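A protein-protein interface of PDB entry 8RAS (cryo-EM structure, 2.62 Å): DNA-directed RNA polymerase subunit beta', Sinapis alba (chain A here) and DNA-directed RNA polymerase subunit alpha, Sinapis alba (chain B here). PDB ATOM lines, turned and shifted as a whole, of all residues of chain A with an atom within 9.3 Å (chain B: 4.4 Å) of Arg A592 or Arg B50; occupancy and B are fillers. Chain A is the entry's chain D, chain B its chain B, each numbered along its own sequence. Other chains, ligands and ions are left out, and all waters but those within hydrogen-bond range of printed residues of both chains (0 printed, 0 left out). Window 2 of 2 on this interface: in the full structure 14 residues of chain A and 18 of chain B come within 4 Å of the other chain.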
ATOM      1  N   PHE A 581      12.245  17.504  -1.019  1.00  0.00           N
ATOM      2  CA  PHE A 581      13.278  18.508  -0.817  1.00  0.00           C
ATOM      3  C   PHE A 581      12.999  19.722  -1.689  1.00  0.00           C
ATOM      4  O   PHE A 581      12.653  19.587  -2.868  1.00  0.00           O
ATOM      5  CB  PHE A 581      14.664  17.941  -1.130  1.00  0.00           C
ATOM      6  CG  PHE A 581      15.142  16.932  -0.127  1.00  0.00           C
ATOM      7  CD1 PHE A 581      15.635  17.337   1.101  1.00  0.00           C
ATOM      8  CD2 PHE A 581      15.096  15.579  -0.411  1.00  0.00           C
ATOM      9  CE1 PHE A 581      16.073  16.411   2.024  1.00  0.00           C
ATOM     10  CE2 PHE A 581      15.534  14.651   0.509  1.00  0.00           C
ATOM     11  CZ  PHE A 581      16.023  15.067   1.727  1.00  0.00           C
ATOM     12  N   SER A 584      18.202  21.010  -4.442  1.00  0.00           N
ATOM     13  CA  SER A 584      19.228  19.972  -4.406  1.00  0.00           C
ATOM     14  C   SER A 584      20.183  20.157  -3.234  1.00  0.00           C
ATOM     15  O   SER A 584      20.706  19.172  -2.696  1.00  0.00           O
ATOM     16  CB  SER A 584      20.008  19.968  -5.718  1.00  0.00           C
ATOM     17  OG  SER A 584      20.867  21.091  -5.796  1.00  0.00           O
ATOM     18  N   TYR A 585      20.430  21.406  -2.833  1.00  0.00           N
ATOM     19  CA  TYR A 585      21.314  21.656  -1.700  1.00  0.00           C
ATOM     20  C   TYR A 585      20.753  21.040  -0.426  1.00  0.00           C
ATOM     21  O   TYR A 585      21.501  20.481   0.381  1.00  0.00           O
ATOM     22  CB  TYR A 585      21.535  23.158  -1.521  1.00  0.00           C
ATOM     23  CG  TYR A 585      21.900  23.878  -2.797  1.00  0.00           C
ATOM     24  CD1 TYR A 585      23.116  23.648  -3.423  1.00  0.00           C
ATOM     25  CD2 TYR A 585      21.027  24.786  -3.378  1.00  0.00           C
ATOM     26  CE1 TYR A 585      23.454  24.301  -4.590  1.00  0.00           C
ATOM     27  CE2 TYR A 585      21.355  25.444  -4.544  1.00  0.00           C
ATOM     28  CZ  TYR A 585      22.569  25.199  -5.146  1.00  0.00           C
ATOM     29  OH  TYR A 585      22.898  25.854  -6.310  1.00  0.00           O
ATOM     30  N   ASP A 586      19.435  21.125  -0.235  1.00  0.00           N
ATOM     31  CA  ASP A 586      18.812  20.498   0.927  1.00  0.00           C
ATOM     32  C   ASP A 586      19.007  18.987   0.909  1.00  0.00           C
ATOM     33  O   ASP A 586      19.294  18.378   1.946  1.00  0.00           O
ATOM     34  CB  ASP A 586      17.325  20.845   0.973  1.00  0.00           C
ATOM     35  CG  ASP A 586      17.056  22.172   1.653  1.00  0.00           C
ATOM     36  OD1 ASP A 586      17.887  22.596   2.484  1.00  0.00           O
ATOM     37  OD2 ASP A 586      16.014  22.792   1.355  1.00  0.00           O
ATOM     38  N   ALA A 587      18.854  18.365  -0.262  1.00  0.00           N
ATOM     39  CA  ALA A 587      19.023  16.919  -0.364  1.00  0.00           C
ATOM     40  C   ALA A 587      20.455  16.500  -0.061  1.00  0.00           C
ATOM     41  O   ALA A 587      20.687  15.532   0.674  1.00  0.00           O
ATOM     42  CB  ALA A 587      18.613  16.441  -1.756  1.00  0.00           C
ATOM     43  N   ILE A 588      21.434  17.218  -0.613  1.00  0.00           N
ATOM     44  CA  ILE A 588      22.823  16.861  -0.344  1.00  0.00           C
ATOM     45  C   ILE A 588      23.175  17.119   1.117  1.00  0.00           C
ATOM     46  O   ILE A 588      23.928  16.355   1.728  1.00  0.00           O
ATOM     47  CB  ILE A 588      23.767  17.588  -1.318  1.00  0.00           C
ATOM     48  CG1 ILE A 588      23.822  16.820  -2.639  1.00  0.00           C
ATOM     49  CG2 ILE A 588      25.163  17.721  -0.742  1.00  0.00           C
ATOM     50  CD1 ILE A 588      23.892  17.672  -3.877  1.00  0.00           C
ATOM     51  N   GLY A 589      22.628  18.183   1.708  1.00  0.00           N
ATOM     52  CA  GLY A 589      22.847  18.415   3.126  1.00  0.00           C
ATOM     53  C   GLY A 589      22.260  17.322   3.999  1.00  0.00           C
ATOM     54  O   GLY A 589      22.856  16.934   5.006  1.00  0.00           O
ATOM     55  N   ALA A 590      21.075  16.826   3.642  1.00  0.00           N
ATOM     56  CA  ALA A 590      20.507  15.691   4.362  1.00  0.00           C
ATOM     57  C   ALA A 590      21.372  14.449   4.190  1.00  0.00           C
ATOM     58  O   ALA A 590      21.525  13.651   5.122  1.00  0.00           O
ATOM     59  CB  ALA A 590      19.082  15.427   3.885  1.00  0.00           C
ATOM     60  N   TYR A 591      21.937  14.265   2.996  1.00  0.00           N
ATOM     61  CA  TYR A 591      22.838  13.140   2.766  1.00  0.00           C
ATOM     62  C   TYR A 591      24.092  13.249   3.624  1.00  0.00           C
ATOM     63  O   TYR A 591      24.597  12.241   4.132  1.00  0.00           O
ATOM     64  CB  TYR A 591      23.205  13.063   1.286  1.00  0.00           C
ATOM     65  CG  TYR A 591      24.218  11.994   0.958  1.00  0.00           C
ATOM     66  CD1 TYR A 591      23.903  10.650   1.088  1.00  0.00           C
ATOM     67  CD2 TYR A 591      25.488  12.330   0.512  1.00  0.00           C
ATOM     68  CE1 TYR A 591      24.824   9.670   0.788  1.00  0.00           C
ATOM     69  CE2 TYR A 591      26.417  11.356   0.210  1.00  0.00           C
ATOM     70  CZ  TYR A 591      26.079  10.028   0.349  1.00  0.00           C
ATOM     71  OH  TYR A 591      26.998   9.050   0.049  1.00  0.00           O
ATOM     72  N   ARG A 592      24.617  14.467   3.783  1.00  0.00           N
ATOM     73  CA  ARG A 592      25.809  14.667   4.601  1.00  0.00           C
ATOM     74  C   ARG A 592      25.540  14.336   6.063  1.00  0.00           C
ATOM     75  O   ARG A 592      26.394  13.761   6.745  1.00  0.00           O
ATOM     76  CB  ARG A 592      26.305  16.105   4.461  1.00  0.00           C
ATOM     77  CG  ARG A 592      27.062  16.377   3.175  1.00  0.00           C
ATOM     78  CD  ARG A 592      27.877  17.654   3.276  1.00  0.00           C
ATOM     79  NE  ARG A 592      27.059  18.843   3.075  1.00  0.00           N
ATOM     80  CZ  ARG A 592      27.032  19.552   1.956  1.00  0.00           C
ATOM     81  NH1 ARG A 592      27.772  19.221   0.910  1.00  0.00           N
ATOM     82  NH2 ARG A 592      26.244  20.621   1.883  1.00  0.00           N
ATOM     83  N   GLN A 593      24.360  14.696   6.562  1.00  0.00           N
ATOM     84  CA  GLN A 593      23.964  14.391   7.928  1.00  0.00           C
ATOM     85  C   GLN A 593      23.432  12.973   8.085  1.00  0.00           C
ATOM     86  O   GLN A 593      22.782  12.676   9.095  1.00  0.00           O
ATOM     87  CB  GLN A 593      22.921  15.401   8.410  1.00  0.00           C
ATOM     88  CG  GLN A 593      23.473  16.795   8.641  1.00  0.00           C
ATOM     89  CD  GLN A 593      22.387  17.845   8.719  1.00  0.00           C
ATOM     90  OE1 GLN A 593      21.228  17.580   8.405  1.00  0.00           O
ATOM     91  NE2 GLN A 593      22.757  19.049   9.139  1.00  0.00           N
ATOM     92  N   LYS A 594      23.682  12.105   7.104  1.00  0.00           N
ATOM     93  CA  LYS A 594      23.331  10.687   7.149  1.00  0.00           C
ATOM     94  C   LYS A 594      21.834  10.453   7.316  1.00  0.00           C
ATOM     95  O   LYS A 594      21.421   9.404   7.819  1.00  0.00           O
ATOM     96  CB  LYS A 594      24.103   9.958   8.254  1.00  0.00           C
ATOM     97  CG  LYS A 594      25.587  10.281   8.296  1.00  0.00           C
ATOM     98  CD  LYS A 594      26.273   9.916   6.993  1.00  0.00           C
ATOM     99  CE  LYS A 594      27.771  10.156   7.075  1.00  0.00           C
ATOM    100  NZ  LYS A 594      28.090  11.450   7.740  1.00  0.00           N
ATOM    101  N   ARG A 595      21.004  11.412   6.906  1.00  0.00           N
ATOM    102  CA  ARG A 595      19.562  11.210   6.959  1.00  0.00           C
ATOM    103  C   ARG A 595      19.071  10.309   5.836  1.00  0.00           C
ATOM    104  O   ARG A 595      18.079   9.592   6.010  1.00  0.00           O
ATOM    105  CB  ARG A 595      18.837  12.553   6.907  1.00  0.00           C
ATOM    106  CG  ARG A 595      19.151  13.468   8.073  1.00  0.00           C
ATOM    107  CD  ARG A 595      18.968  14.923   7.690  1.00  0.00           C
ATOM    108  NE  ARG A 595      18.859  15.780   8.863  1.00  0.00           N
ATOM    109  CZ  ARG A 595      17.721  16.059   9.482  1.00  0.00           C
ATOM    110  NH1 ARG A 595      16.567  15.568   9.062  1.00  0.00           N
ATOM    111  NH2 ARG A 595      17.742  16.852  10.549  1.00  0.00           N
ATOM    112  N   ILE A 596      19.739  10.336   4.682  1.00  0.00           N
ATOM    113  CA  ILE A 596      19.367   9.523   3.533  1.00  0.00           C
ATOM    114  C   ILE A 596      20.622   8.880   2.961  1.00  0.00           C
ATOM    115  O   ILE A 596      21.745   9.325   3.207  1.00  0.00           O
ATOM    116  CB  ILE A 596      18.642  10.345   2.444  1.00  0.00           C
ATOM    117  CG1 ILE A 596      19.486  11.554   2.043  1.00  0.00           C
ATOM    118  CG2 ILE A 596      17.270  10.784   2.926  1.00  0.00           C
ATOM    119  CD1 ILE A 596      18.791  12.485   1.090  1.00  0.00           C
ATOM    120  N   ASN A 597      20.415   7.819   2.187  1.00  0.00           N
ATOM    121  CA  ASN A 597      21.509   7.095   1.563  1.00  0.00           C
ATOM    122  C   ASN A 597      21.806   7.674   0.181  1.00  0.00           C
ATOM    123  O   ASN A 597      21.150   8.606  -0.287  1.00  0.00           O
ATOM    124  CB  ASN A 597      21.182   5.606   1.475  1.00  0.00           C
ATOM    125  CG  ASN A 597      21.077   4.952   2.835  1.00  0.00           C
ATOM    126  OD1 ASN A 597      21.672   5.415   3.806  1.00  0.00           O
ATOM    127  ND2 ASN A 597      20.318   3.867   2.913  1.00  0.00           N
ATOM    128  N   LEU A 598      22.815   7.109  -0.484  1.00  0.00           N
ATOM    129  CA  LEU A 598      23.174   7.579  -1.818  1.00  0.00           C
ATOM    130  C   LEU A 598      22.132   7.189  -2.857  1.00  0.00           C
ATOM    131  O   LEU A 598      21.951   7.905  -3.849  1.00  0.00           O
ATOM    132  CB  LEU A 598      24.544   7.035  -2.216  1.00  0.00           C
ATOM    133  CG  LEU A 598      25.185   7.685  -3.443  1.00  0.00           C
ATOM    134  CD1 LEU A 598      25.680   9.080  -3.106  1.00  0.00           C
ATOM    135  CD2 LEU A 598      26.314   6.823  -3.978  1.00  0.00           C
ATOM    136  N   VAL A 656      20.333  11.017  -4.538  1.00  0.00           N
ATOM    137  CA  VAL A 656      21.390  11.992  -4.299  1.00  0.00           C
ATOM    138  C   VAL A 656      22.499  11.850  -5.333  1.00  0.00           C
ATOM    139  O   VAL A 656      23.196  12.821  -5.636  1.00  0.00           O
ATOM    140  CB  VAL A 656      21.928  11.856  -2.861  1.00  0.00           C
ATOM    141  CG1 VAL A 656      22.971  12.920  -2.569  1.00  0.00           C
ATOM    142  CG2 VAL A 656      20.794  11.962  -1.869  1.00  0.00           C
ATOM    143  N   SER A 660      24.011  14.798  -7.509  1.00  0.00           N
ATOM    144  CA  SER A 660      25.424  15.112  -7.337  1.00  0.00           C
ATOM    145  C   SER A 660      26.144  15.195  -8.677  1.00  0.00           C
ATOM    146  O   SER A 660      26.965  16.091  -8.886  1.00  0.00           O
ATOM    147  CB  SER A 660      26.083  14.070  -6.437  1.00  0.00           C
ATOM    148  OG  SER A 660      25.475  14.047  -5.161  1.00  0.00           O
ATOM    149  N   ARG A 663      24.972  18.424 -10.377  1.00  0.00           N
ATOM    150  CA  ARG A 663      25.563  19.581  -9.722  1.00  0.00           C
ATOM    151  C   ARG A 663      27.048  19.689 -10.013  1.00  0.00           C
ATOM    152  O   ARG A 663      27.574  20.794 -10.145  1.00  0.00           O
ATOM    153  CB  ARG A 663      25.336  19.535  -8.215  1.00  0.00           C
ATOM    154  CG  ARG A 663      24.210  20.423  -7.749  1.00  0.00           C
ATOM    155  CD  ARG A 663      24.780  21.586  -6.944  1.00  0.00           C
ATOM    156  NE  ARG A 663      25.733  21.159  -5.928  1.00  0.00           N
ATOM    157  CZ  ARG A 663      25.401  20.779  -4.701  1.00  0.00           C
ATOM    158  NH1 ARG A 663      24.145  20.802  -4.289  1.00  0.00           N
ATOM    159  NH2 ARG A 663      26.355  20.379  -3.866  1.00  0.00           N
ATOM    160  N   GLU A 667      28.258  23.017 -11.698  1.00  0.00           N
ATOM    161  CA  GLU A 667      29.187  23.845 -10.948  1.00  0.00           C
ATOM    162  C   GLU A 667      30.512  23.988 -11.671  1.00  0.00           C
ATOM    163  O   GLU A 667      31.135  25.049 -11.593  1.00  0.00           O
ATOM    164  CB  GLU A 667      29.404  23.258  -9.555  1.00  0.00           C
ATOM    165  CG  GLU A 667      28.339  23.644  -8.544  1.00  0.00           C
ATOM    166  CD  GLU A 667      28.746  23.319  -7.121  1.00  0.00           C
ATOM    167  OE1 GLU A 667      29.791  22.661  -6.937  1.00  0.00           O
ATOM    168  OE2 GLU A 667      28.020  23.719  -6.186  1.00  0.00           O
ATOM    169  N   GLY B  46      40.876  20.169  10.704  1.00  0.00           N
ATOM    170  CA  GLY B  46      39.899  20.400   9.654  1.00  0.00           C
ATOM    171  C   GLY B  46      38.784  19.375   9.653  1.00  0.00           C
ATOM    172  O   GLY B  46      37.617  19.722   9.472  1.00  0.00           O
ATOM    173  N   ILE B  47      39.124  18.102   9.863  1.00  0.00           N
ATOM    174  CA  ILE B  47      38.105  17.056   9.892  1.00  0.00           C
ATOM    175  C   ILE B  47      37.143  17.283  11.053  1.00  0.00           C
ATOM    176  O   ILE B  47      35.913  17.260  10.884  1.00  0.00           O
ATOM    177  CB  ILE B  47      38.770  15.669   9.969  1.00  0.00           C
ATOM    178  CG1 ILE B  47      39.453  15.337   8.641  1.00  0.00           C
ATOM    179  CG2 ILE B  47      37.750  14.603  10.328  1.00  0.00           C
ATOM    180  CD1 ILE B  47      40.608  14.368   8.768  1.00  0.00           C
ATOM    181  N   ALA B  48      37.689  17.524  12.249  1.00  0.00           N
ATOM    182  CA  ALA B  48      36.836  17.741  13.413  1.00  0.00           C
ATOM    183  C   ALA B  48      35.978  18.989  13.247  1.00  0.00           C
ATOM    184  O   ALA B  48      34.781  18.975  13.561  1.00  0.00           O
ATOM    185  CB  ALA B  48      37.688  17.837  14.676  1.00  0.00           C
ATOM    186  N   MET B  49      36.569  20.076  12.743  1.00  0.00           N
ATOM    187  CA  MET B  49      35.827  21.319  12.576  1.00  0.00           C
ATOM    188  C   MET B  49      34.740  21.180  11.523  1.00  0.00           C
ATOM    189  O   MET B  49      33.646  21.722  11.689  1.00  0.00           O
ATOM    190  CB  MET B  49      36.781  22.457  12.214  1.00  0.00           C
ATOM    191  CG  MET B  49      37.619  22.965  13.375  1.00  0.00           C
ATOM    192  SD  MET B  49      36.662  23.860  14.611  1.00  0.00           S
ATOM    193  CE  MET B  49      36.113  25.270  13.659  1.00  0.00           C
ATOM    194  N   ARG B  50      35.017  20.468  10.428  1.00  0.00           N
ATOM    195  CA  ARG B  50      33.991  20.270   9.413  1.00  0.00           C
ATOM    196  C   ARG B  50      32.833  19.450   9.958  1.00  0.00           C
ATOM    197  O   ARG B  50      31.666  19.778   9.713  1.00  0.00           O
ATOM    198  CB  ARG B  50      34.591  19.600   8.177  1.00  0.00           C
ATOM    199  CG  ARG B  50      33.572  19.309   7.092  1.00  0.00           C
ATOM    200  CD  ARG B  50      34.235  19.025   5.758  1.00  0.00           C
ATOM    201  NE  ARG B  50      33.257  18.718   4.721  1.00  0.00           N
ATOM    202  CZ  ARG B  50      32.584  17.579   4.634  1.00  0.00           C
ATOM    203  NH1 ARG B  50      32.769  16.598   5.500  1.00  0.00           N
ATOM    204  NH2 ARG B  50      31.701  17.421   3.652  1.00  0.00           N
ATOM    205  N   ARG B  51      33.129  18.386  10.710  1.00  0.00           N
ATOM    206  CA  ARG B  51      32.048  17.596  11.293  1.00  0.00           C
ATOM    207  C   ARG B  51      31.224  18.427  12.273  1.00  0.00           C
ATOM    208  O   ARG B  51      29.986  18.363  12.269  1.00  0.00           O
ATOM    209  CB  ARG B  51      32.612  16.350  11.975  1.00  0.00           C
ATOM    210  CG  ARG B  51      31.536  15.444  12.535  1.00  0.00           C
ATOM    211  CD  ARG B  51      31.868  13.975  12.373  1.00  0.00           C
ATOM    212  NE  ARG B  51      30.820  13.147  12.957  1.00  0.00           N
ATOM    213  CZ  ARG B  51      29.668  12.871  12.362  1.00  0.00           C
ATOM    214  NH1 ARG B  51      29.414  13.272  11.128  1.00  0.00           N
ATOM    215  NH2 ARG B  51      28.748  12.172  13.020  1.00  0.00           N
ATOM    216  N   ALA B  52      31.896  19.223  13.111  1.00  0.00           N
ATOM    217  CA  ALA B  52      31.184  20.073  14.060  1.00  0.00           C
ATOM    218  C   ALA B  52      30.325  21.109  13.347  1.00  0.00           C
ATOM    219  O   ALA B  52      29.169  21.326  13.722  1.00  0.00           O
ATOM    220  CB  ALA B  52      32.177  20.756  15.000  1.00  0.00           C
ATOM    221  N   LEU B  53      30.866  21.745  12.308  1.00  0.00           N
ATOM    222  CA  LEU B  53      30.109  22.745  11.567  1.00  0.00           C
ATOM    223  C   LEU B  53      28.892  22.129  10.897  1.00  0.00           C
ATOM    224  O   LEU B  53      27.812  22.731  10.878  1.00  0.00           O
ATOM    225  CB  LEU B  53      31.004  23.415  10.525  1.00  0.00           C
ATOM    226  CG  LEU B  53      32.025  24.434  11.023  1.00  0.00           C
ATOM    227  CD1 LEU B  53      33.174  24.547  10.041  1.00  0.00           C
ATOM    228  CD2 LEU B  53      31.370  25.779  11.242  1.00  0.00           C
ATOM    229  N   LEU B  54      29.044  20.930  10.338  1.00  0.00           N
ATOM    230  CA  LEU B  54      27.944  20.326   9.602  1.00  0.00           C
ATOM    231  C   LEU B  54      26.868  19.752  10.514  1.00  0.00           C
ATOM    232  O   LEU B  54      25.701  19.699  10.113  1.00  0.00           O
ATOM    233  CB  LEU B  54      28.475  19.245   8.662  1.00  0.00           C
ATOM    234  CG  LEU B  54      29.305  19.765   7.485  1.00  0.00           C
ATOM    235  CD1 LEU B  54      29.708  18.629   6.565  1.00  0.00           C
ATOM    236  CD2 LEU B  54      28.545  20.838   6.719  1.00  0.00           C
ATOM    237  N   GLN B 180      25.517  25.675   5.459  1.00  0.00           N
ATOM    238  CA  GLN B 180      25.155  24.939   4.251  1.00  0.00           C
ATOM    239  C   GLN B 180      26.290  24.039   3.779  1.00  0.00           C
ATOM    240  O   GLN B 180      26.050  22.909   3.340  1.00  0.00           O
ATOM    241  CB  GLN B 180      24.753  25.915   3.147  1.00  0.00           C
ATOM    242  CG  GLN B 180      23.837  27.030   3.612  1.00  0.00           C
ATOM    243  CD  GLN B 180      22.378  26.630   3.593  1.00  0.00           C
ATOM    244  OE1 GLN B 180      21.915  25.883   4.455  1.00  0.00           O
ATOM    245  NE2 GLN B 180      21.642  27.124   2.605  1.00  0.00           N
ATOM    246  N   ASN B 181      27.528  24.518   3.857  1.00  0.00           N
ATOM    247  CA  ASN B 181      28.667  23.739   3.396  1.00  0.00           C
ATOM    248  C   ASN B 181      29.903  24.154   4.178  1.00  0.00           C
ATOM    249  O   ASN B 181      29.969  25.248   4.742  1.00  0.00           O
ATOM    250  CB  ASN B 181      28.890  23.918   1.891  1.00  0.00           C
ATOM    251  CG  ASN B 181      29.799  22.859   1.305  1.00  0.00           C
ATOM    252  OD1 ASN B 181      29.993  21.797   1.895  1.00  0.00           O
ATOM    253  ND2 ASN B 181      30.363  23.143   0.139  1.00  0.00           N
ATOM    254  N   ALA B 182      30.888  23.260   4.204  1.00  0.00           N
ATOM    255  CA  ALA B 182      32.149  23.523   4.879  1.00  0.00           C
ATOM    256  C   ALA B 182      33.246  22.706   4.215  1.00  0.00           C
ATOM    257  O   ALA B 182      33.017  21.565   3.804  1.00  0.00           O
ATOM    258  CB  ALA B 182      32.070  23.190   6.372  1.00  0.00           C
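O of Leu B54 sits at hydrogen-bond distance from NE2 of Gln A593 (3.2 Å). The backbone carbonyl oxygen (O) of Gln B180 is in hydrogen-bond range of the guanidinium group (NH2) of Arg A592, 2.7 Å away.
The guanidinium group (NE) of Arg B50 sits at hydrogen-bond distance from the backbone carbonyl oxygen (O) of Ala B182. The backbone carbonyl oxygen of Arg A592 lies within hydrogen-bond range of the side-chain amino group of Lys A594. The guanidinium group of Arg A595 is in hydrogen-bond range of the side-chain amide oxygen of Gln A593 (3.0 Å).
Among the printed residues, merely in contact across the chains: Arg A592 with Asn B181, Arg A592 with Arg B50 and Arg A592 with Leu B54.
Of chain B, only Arg B50, Leu B54, Gln B180 and Asn B181 come within 4 Å of Arg A592. Arg B50 touches one residue of chain A. No residue of chain A comes within 4 Å of Ala B52. Ala B182 touches none of the printed residues of chain A. Of the printed residues of chain B, Gln A593 touches Leu B54 (3.2 Å). Of the printed residues of chain A, Leu B54 touches Arg A592 and Gln A593. Printed residues of chain A within 4 Å of Gln B180: Arg A592. Printed residues of chain A within 4 Å of Asn B181: Arg A592. Ile A596 touches none of the printed residues of chain B. The nearest residue of chain A that does not touch Arg B50 is Lys A594 (7.3 Å). The nearest printed residue of chain A that does not touch Leu B54 is Gly A589 (6.5 Å).
Printed residues of chain B that touch a printed residue of chain A: Arg B50, Leu B54, Gln B180 and Asn B181. Hydrophobic or aromatic side chains of chain B that line the printed part of chain A: Leu B54. Of the 20 printed residues of chain A, 2 touch a printed residue of chain B. Among the printed residues, 5 pairs touch across the chains.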
